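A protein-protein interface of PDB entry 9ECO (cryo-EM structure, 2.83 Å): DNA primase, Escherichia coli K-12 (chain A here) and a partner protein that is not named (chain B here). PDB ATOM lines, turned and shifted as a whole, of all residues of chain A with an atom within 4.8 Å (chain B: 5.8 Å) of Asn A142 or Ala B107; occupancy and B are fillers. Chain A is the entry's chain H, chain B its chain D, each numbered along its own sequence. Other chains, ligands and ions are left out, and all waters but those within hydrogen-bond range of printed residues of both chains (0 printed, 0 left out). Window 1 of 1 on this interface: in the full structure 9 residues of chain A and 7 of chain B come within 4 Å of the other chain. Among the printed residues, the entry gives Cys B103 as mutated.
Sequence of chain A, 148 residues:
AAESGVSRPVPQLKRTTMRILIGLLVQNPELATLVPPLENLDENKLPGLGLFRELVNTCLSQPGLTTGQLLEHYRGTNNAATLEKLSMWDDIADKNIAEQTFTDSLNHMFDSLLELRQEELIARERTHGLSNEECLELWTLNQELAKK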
ATOM      1  N   GLN A 118      -1.798 -11.047  -2.896  1.00  0.00           N
ATOM      2  CA  GLN A 118      -0.599 -10.774  -3.680  1.00  0.00           C
ATOM      3  C   GLN A 118       0.581 -10.405  -2.791  1.00  0.00           C
ATOM      4  O   GLN A 118       1.726 -10.730  -3.121  1.00  0.00           O
ATOM      5  CB  GLN A 118      -0.871  -9.664  -4.695  1.00  0.00           C
ATOM      6  CG  GLN A 118      -1.232  -8.326  -4.081  1.00  0.00           C
ATOM      7  CD  GLN A 118      -1.495  -7.263  -5.128  1.00  0.00           C
ATOM      8  OE1 GLN A 118      -1.992  -7.556  -6.216  1.00  0.00           O
ATOM      9  NE2 GLN A 118      -1.164  -6.019  -4.804  1.00  0.00           N
ATOM     10  N   LEU A 138       0.318 -13.448 -10.602  1.00  0.00           N
ATOM     11  CA  LEU A 138       0.517 -12.138  -9.990  1.00  0.00           C
ATOM     12  C   LEU A 138       0.226 -11.018 -10.978  1.00  0.00           C
ATOM     13  O   LEU A 138      -0.433 -10.028 -10.636  1.00  0.00           O
ATOM     14  CB  LEU A 138       1.953 -12.014  -9.469  1.00  0.00           C
ATOM     15  CG  LEU A 138       2.236 -12.405  -8.019  1.00  0.00           C
ATOM     16  CD1 LEU A 138       3.739 -12.392  -7.771  1.00  0.00           C
ATOM     17  CD2 LEU A 138       1.551 -11.446  -7.053  1.00  0.00           C
ATOM     18  N   TRP A 139       0.713 -11.155 -12.212  1.00  0.00           N
ATOM     19  CA  TRP A 139       0.457 -10.132 -13.217  1.00  0.00           C
ATOM     20  C   TRP A 139      -1.039  -9.942 -13.419  1.00  0.00           C
ATOM     21  O   TRP A 139      -1.519  -8.810 -13.548  1.00  0.00           O
ATOM     22  CB  TRP A 139       1.131 -10.512 -14.534  1.00  0.00           C
ATOM     23  CG  TRP A 139       0.764  -9.608 -15.657  1.00  0.00           C
ATOM     24  CD1 TRP A 139       0.228  -9.962 -16.859  1.00  0.00           C
ATOM     25  CD2 TRP A 139       0.911  -8.186 -15.686  1.00  0.00           C
ATOM     26  NE1 TRP A 139       0.030  -8.846 -17.636  1.00  0.00           N
ATOM     27  CE2 TRP A 139       0.442  -7.742 -16.937  1.00  0.00           C
ATOM     28  CE3 TRP A 139       1.394  -7.244 -14.773  1.00  0.00           C
ATOM     29  CZ2 TRP A 139       0.443  -6.396 -17.299  1.00  0.00           C
ATOM     30  CZ3 TRP A 139       1.393  -5.912 -15.132  1.00  0.00           C
ATOM     31  CH2 TRP A 139       0.921  -5.499 -16.384  1.00  0.00           C
ATOM     32  N   THR A 140      -1.791 -11.042 -13.455  1.00  0.00           N
ATOM     33  CA  THR A 140      -3.241 -10.951 -13.555  1.00  0.00           C
ATOM     34  C   THR A 140      -3.862 -10.337 -12.308  1.00  0.00           C
ATOM     35  O   THR A 140      -4.970  -9.795 -12.386  1.00  0.00           O
ATOM     36  CB  THR A 140      -3.836 -12.338 -13.795  1.00  0.00           C
ATOM     37  OG1 THR A 140      -3.448 -13.216 -12.730  1.00  0.00           O
ATOM     38  CG2 THR A 140      -3.350 -12.905 -15.120  1.00  0.00           C
ATOM     39  N   LEU A 141      -3.179 -10.403 -11.167  1.00  0.00           N
ATOM     40  CA  LEU A 141      -3.721  -9.877  -9.921  1.00  0.00           C
ATOM     41  C   LEU A 141      -3.598  -8.364  -9.810  1.00  0.00           C
ATOM     42  O   LEU A 141      -4.130  -7.789  -8.854  1.00  0.00           O
ATOM     43  CB  LEU A 141      -3.024 -10.527  -8.720  1.00  0.00           C
ATOM     44  CG  LEU A 141      -3.175 -12.037  -8.504  1.00  0.00           C
ATOM     45  CD1 LEU A 141      -3.106 -12.365  -7.019  1.00  0.00           C
ATOM     46  CD2 LEU A 141      -4.460 -12.583  -9.114  1.00  0.00           C
ATOM     47  N   ASN A 142      -2.915  -7.706 -10.747  1.00  0.00           N
ATOM     48  CA  ASN A 142      -2.770  -6.258 -10.711  1.00  0.00           C
ATOM     49  C   ASN A 142      -3.873  -5.523 -11.460  1.00  0.00           C
ATOM     50  O   ASN A 142      -4.078  -4.329 -11.209  1.00  0.00           O
ATOM     51  CB  ASN A 142      -1.413  -5.847 -11.294  1.00  0.00           C
ATOM     52  CG  ASN A 142      -0.254  -6.232 -10.396  1.00  0.00           C
ATOM     53  OD1 ASN A 142      -0.417  -7.000  -9.449  1.00  0.00           O
ATOM     54  ND2 ASN A 142       0.926  -5.698 -10.690  1.00  0.00           N
ATOM     55  N   GLN A 143      -4.585  -6.198 -12.365  1.00  0.00           N
ATOM     56  CA  GLN A 143      -5.652  -5.531 -13.105  1.00  0.00           C
ATOM     57  C   GLN A 143      -6.766  -5.072 -12.174  1.00  0.00           C
ATOM     58  O   GLN A 143      -7.269  -3.949 -12.302  1.00  0.00           O
ATOM     59  CB  GLN A 143      -6.207  -6.465 -14.180  1.00  0.00           C
ATOM     60  CG  GLN A 143      -5.338  -6.556 -15.421  1.00  0.00           C
ATOM     61  CD  GLN A 143      -4.029  -7.271 -15.163  1.00  0.00           C
ATOM     62  OE1 GLN A 143      -3.710  -7.609 -14.023  1.00  0.00           O
ATOM     63  NE2 GLN A 143      -3.262  -7.506 -16.222  1.00  0.00           N
ATOM     64  N   GLU A 144      -7.163  -5.924 -11.227  1.00  0.00           N
ATOM     65  CA  GLU A 144      -8.227  -5.546 -10.301  1.00  0.00           C
ATOM     66  C   GLU A 144      -7.826  -4.333  -9.470  1.00  0.00           C
ATOM     67  O   GLU A 144      -8.637  -3.425  -9.253  1.00  0.00           O
ATOM     68  CB  GLU A 144      -8.590  -6.722  -9.393  1.00  0.00           C
ATOM     69  CG  GLU A 144      -7.403  -7.496  -8.837  1.00  0.00           C
ATOM     70  CD  GLU A 144      -7.056  -8.712  -9.673  1.00  0.00           C
ATOM     71  OE1 GLU A 144      -6.978  -8.579 -10.913  1.00  0.00           O
ATOM     72  OE2 GLU A 144      -6.871  -9.803  -9.092  1.00  0.00           O
ATOM     73  N   LEU A 145      -6.579  -4.298  -8.998  1.00  0.00           N
ATOM     74  CA  LEU A 145      -6.100  -3.154  -8.233  1.00  0.00           C
ATOM     75  C   LEU A 145      -5.909  -1.914  -9.093  1.00  0.00           C
ATOM     76  O   LEU A 145      -5.682  -0.830  -8.543  1.00  0.00           O
ATOM     77  CB  LEU A 145      -4.784  -3.503  -7.534  1.00  0.00           C
ATOM     78  CG  LEU A 145      -4.871  -4.343  -6.254  1.00  0.00           C
ATOM     79  CD1 LEU A 145      -5.755  -3.672  -5.208  1.00  0.00           C
ATOM     80  CD2 LEU A 145      -5.379  -5.742  -6.558  1.00  0.00           C
ATOM     81  N   ALA A 146      -5.988  -2.041 -10.414  1.00  0.00           N
ATOM     82  CA  ALA A 146      -5.902  -0.914 -11.334  1.00  0.00           C
ATOM     83  C   ALA A 146      -7.028  -0.978 -12.354  1.00  0.00           C
ATOM     84  O   ALA A 146      -6.863  -0.602 -13.518  1.00  0.00           O
ATOM     85  CB  ALA A 146      -4.544  -0.880 -12.031  1.00  0.00           C
ATOM     86  N   LEU B  84       4.900  -6.634 -18.790  1.00  0.00           N
ATOM     87  CA  LEU B  84       5.752  -7.171 -17.733  1.00  0.00           C
ATOM     88  C   LEU B  84       6.541  -8.382 -18.214  1.00  0.00           C
ATOM     89  O   LEU B  84       7.742  -8.498 -17.942  1.00  0.00           O
ATOM     90  CB  LEU B  84       4.902  -7.542 -16.517  1.00  0.00           C
ATOM     91  CG  LEU B  84       5.620  -8.259 -15.370  1.00  0.00           C
ATOM     92  CD1 LEU B  84       6.803  -7.445 -14.873  1.00  0.00           C
ATOM     93  CD2 LEU B  84       4.651  -8.540 -14.232  1.00  0.00           C
ATOM     94  N   GLY B 102      13.085  -8.011  -9.922  1.00  0.00           N
ATOM     95  CA  GLY B 102      12.562  -9.249 -10.462  1.00  0.00           C
ATOM     96  C   GLY B 102      11.071  -9.152 -10.682  1.00  0.00           C
ATOM     97  O   GLY B 102      10.519  -8.059 -10.822  1.00  0.00           O
ATOM     98  N   CYS B 103      10.422 -10.317 -10.711  1.00  0.00           N
ATOM     99  CA  CYS B 103       8.974 -10.356 -10.897  1.00  0.00           C
ATOM    100  C   CYS B 103       8.269  -9.507  -9.845  1.00  0.00           C
ATOM    101  O   CYS B 103       7.357  -8.734 -10.161  1.00  0.00           O
ATOM    102  CB  CYS B 103       8.482 -11.805 -10.843  1.00  0.00           C
ATOM    103  SG  CYS B 103       8.121 -12.543 -12.458  1.00  0.00           S
ATOM    104  N   ALA B 104       8.685  -9.634  -8.584  1.00  0.00           N
ATOM    105  CA  ALA B 104       8.060  -8.860  -7.516  1.00  0.00           C
ATOM    106  C   ALA B 104       8.347  -7.372  -7.673  1.00  0.00           C
ATOM    107  O   ALA B 104       7.437  -6.540  -7.572  1.00  0.00           O
ATOM    108  CB  ALA B 104       8.546  -9.360  -6.156  1.00  0.00           C
ATOM    109  N   TYR B 105       9.609  -7.015  -7.921  1.00  0.00           N
ATOM    110  CA  TYR B 105       9.964  -5.606  -8.047  1.00  0.00           C
ATOM    111  C   TYR B 105       9.218  -4.958  -9.205  1.00  0.00           C
ATOM    112  O   TYR B 105       8.634  -3.878  -9.058  1.00  0.00           O
ATOM    113  CB  TYR B 105      11.473  -5.462  -8.235  1.00  0.00           C
ATOM    114  CG  TYR B 105      12.006  -4.092  -7.887  1.00  0.00           C
ATOM    115  CD1 TYR B 105      11.915  -3.042  -8.791  1.00  0.00           C
ATOM    116  CD2 TYR B 105      12.599  -3.847  -6.657  1.00  0.00           C
ATOM    117  CE1 TYR B 105      12.400  -1.787  -8.479  1.00  0.00           C
ATOM    118  CE2 TYR B 105      13.087  -2.594  -6.336  1.00  0.00           C
ATOM    119  CZ  TYR B 105      12.985  -1.568  -7.252  1.00  0.00           C
ATOM    120  OH  TYR B 105      13.470  -0.320  -6.938  1.00  0.00           O
ATOM    121  N   LEU B 106       9.219  -5.613 -10.367  1.00  0.00           N
ATOM    122  CA  LEU B 106       8.524  -5.060 -11.523  1.00  0.00           C
ATOM    123  C   LEU B 106       7.014  -5.067 -11.322  1.00  0.00           C
ATOM    124  O   LEU B 106       6.322  -4.168 -11.810  1.00  0.00           O
ATOM    125  CB  LEU B 106       8.903  -5.839 -12.781  1.00  0.00           C
ATOM    126  CG  LEU B 106      10.406  -5.955 -13.049  1.00  0.00           C
ATOM    127  CD1 LEU B 106      10.694  -7.105 -13.999  1.00  0.00           C
ATOM    128  CD2 LEU B 106      10.955  -4.648 -13.597  1.00  0.00           C
ATOM    129  N   ALA B 107       6.485  -6.071 -10.621  1.00  0.00           N
ATOM    130  CA  ALA B 107       5.065  -6.062 -10.288  1.00  0.00           C
ATOM    131  C   ALA B 107       4.724  -4.880  -9.390  1.00  0.00           C
ATOM    132  O   ALA B 107       3.688  -4.230  -9.570  1.00  0.00           O
ATOM    133  CB  ALA B 107       4.672  -7.377  -9.618  1.00  0.00           C
ATOM    134  N   GLU B 108       5.587  -4.586  -8.414  1.00  0.00           N
ATOM    135  CA  GLU B 108       5.362  -3.432  -7.551  1.00  0.00           C
ATOM    136  C   GLU B 108       5.405  -2.137  -8.352  1.00  0.00           C
ATOM    137  O   GLU B 108       4.735  -1.158  -8.000  1.00  0.00           O
ATOM    138  CB  GLU B 108       6.404  -3.404  -6.434  1.00  0.00           C
ATOM    139  CG  GLU B 108       6.122  -2.379  -5.348  1.00  0.00           C
ATOM    140  CD  GLU B 108       7.247  -2.275  -4.337  1.00  0.00           C
ATOM    141  OE1 GLU B 108       8.311  -2.886  -4.566  1.00  0.00           O
ATOM    142  OE2 GLU B 108       7.064  -1.584  -3.313  1.00  0.00           O
ATOM    143  N   LEU B 109       6.193  -2.110  -9.429  1.00  0.00           N
ATOM    144  CA  LEU B 109       6.284  -0.910 -10.254  1.00  0.00           C
ATOM    145  C   LEU B 109       4.911  -0.507 -10.776  1.00  0.00           C
ATOM    146  O   LEU B 109       4.516   0.662 -10.688  1.00  0.00           O
ATOM    147  CB  LEU B 109       7.252  -1.149 -11.415  1.00  0.00           C
ATOM    148  CG  LEU B 109       8.651  -0.532 -11.324  1.00  0.00           C
ATOM    149  CD1 LEU B 109       8.587   0.979 -11.187  1.00  0.00           C
ATOM    150  CD2 LEU B 109       9.435  -1.140 -10.171  1.00  0.00           C
ATOM    151  N   SER B 110       4.164  -1.468 -11.323  1.00  0.00           N
ATOM    152  CA  SER B 110       2.820  -1.193 -11.813  1.00  0.00           C
ATOM    153  C   SER B 110       1.798  -1.079 -10.693  1.00  0.00           C
ATOM    154  O   SER B 110       0.744  -0.465 -10.893  1.00  0.00           O
ATOM    155  CB  SER B 110       2.379  -2.288 -12.785  1.00  0.00           C
ATOM    156  OG  SER B 110       1.055  -2.065 -13.235  1.00  0.00           O
ATOM    157  N   LYS B 111       2.083  -1.652  -9.522  1.00  0.00           N
ATOM    158  CA  LYS B 111       1.106  -1.650  -8.441  1.00  0.00           C
ATOM    159  C   LYS B 111       0.836  -0.236  -7.939  1.00  0.00           C
ATOM    160  O   LYS B 111      -0.307   0.105  -7.615  1.00  0.00           O
ATOM    161  CB  LYS B 111       1.595  -2.542  -7.301  1.00  0.00           C
ATOM    162  CG  LYS B 111       0.743  -2.475  -6.046  1.00  0.00           C
ATOM    163  CD  LYS B 111       1.189  -3.509  -5.027  1.00  0.00           C
ATOM    164  CE  LYS B 111       0.841  -3.080  -3.614  1.00  0.00           C
ATOM    165  NZ  LYS B 111       1.312  -4.065  -2.601  1.00  0.00           N
ATOM    166  N   ASN B 112       1.870   0.599  -7.871  1.00  0.00           N
ATOM    167  CA  ASN B 112       1.750   1.939  -7.312  1.00  0.00           C
ATOM    168  C   ASN B 112       1.290   2.975  -8.329  1.00  0.00           C
ATOM    169  O   ASN B 112       1.133   4.146  -7.967  1.00  0.00           O
ATOM    170  CB  ASN B 112       3.088   2.381  -6.714  1.00  0.00           C
ATOM    171  CG  ASN B 112       3.932   3.170  -7.695  1.00  0.00           C
ATOM    172  OD1 ASN B 112       4.097   2.774  -8.850  1.00  0.00           O
ATOM    173  ND2 ASN B 112       4.463   4.300  -7.243  1.00  0.00           N
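Among the printed residues, pairs that only touch across the chains: Gln A118 with Lys B111 (3.4 Å) and Trp A139 with Leu B84 (3.5 Å).
Asn A142 touches one residue of chain B. Ala B107 touches just one residue of chain A: Asn A142 (3.3 Å). Of the printed residues of chain A, Lys B111 touches Gln A118 (3.4 Å). Of the printed residues of chain B, Trp A139 touches Leu B84. Printed residues of chain B within 4 Å of Gln A118: Lys B111 (3.4 Å). Printed residues of chain A within 4 Å of Leu B84: Trp A139 (3.5 Å). Leu B109 touches none of the printed residues of chain A. Glu A144 touches none of the printed residues of chain B. The nearest printed residue of chain A that does not touch Ala B107 is Leu A138 (5.4 Å).
Of the 10 printed residues of chain A, 3 touch a printed residue of chain B. Printed residues of chain A that touch a printed residue of chain B: Gln A118, Trp A139 and Asn A142. Hydrophobic or aromatic side chains of chain A that line the printed part of chain B: Trp A139. Among the printed residues, 3 pairs touch across the chains.
The side-chain amide oxygen (OE1) of Gln A118 lies close to the backbone carbonyl oxygen (O) of Leu A141. OD1 of Asn A142 sits close to O of Leu A138 (3.3 Å). OE1 of Gln A143 lies close to O of Trp A139 (2.5 Å).
The backbone carbonyl oxygen of Ala B107 sits at hydrogen-bond distance from the side-chain amide nitrogen of Asn A142 (3.3 Å).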
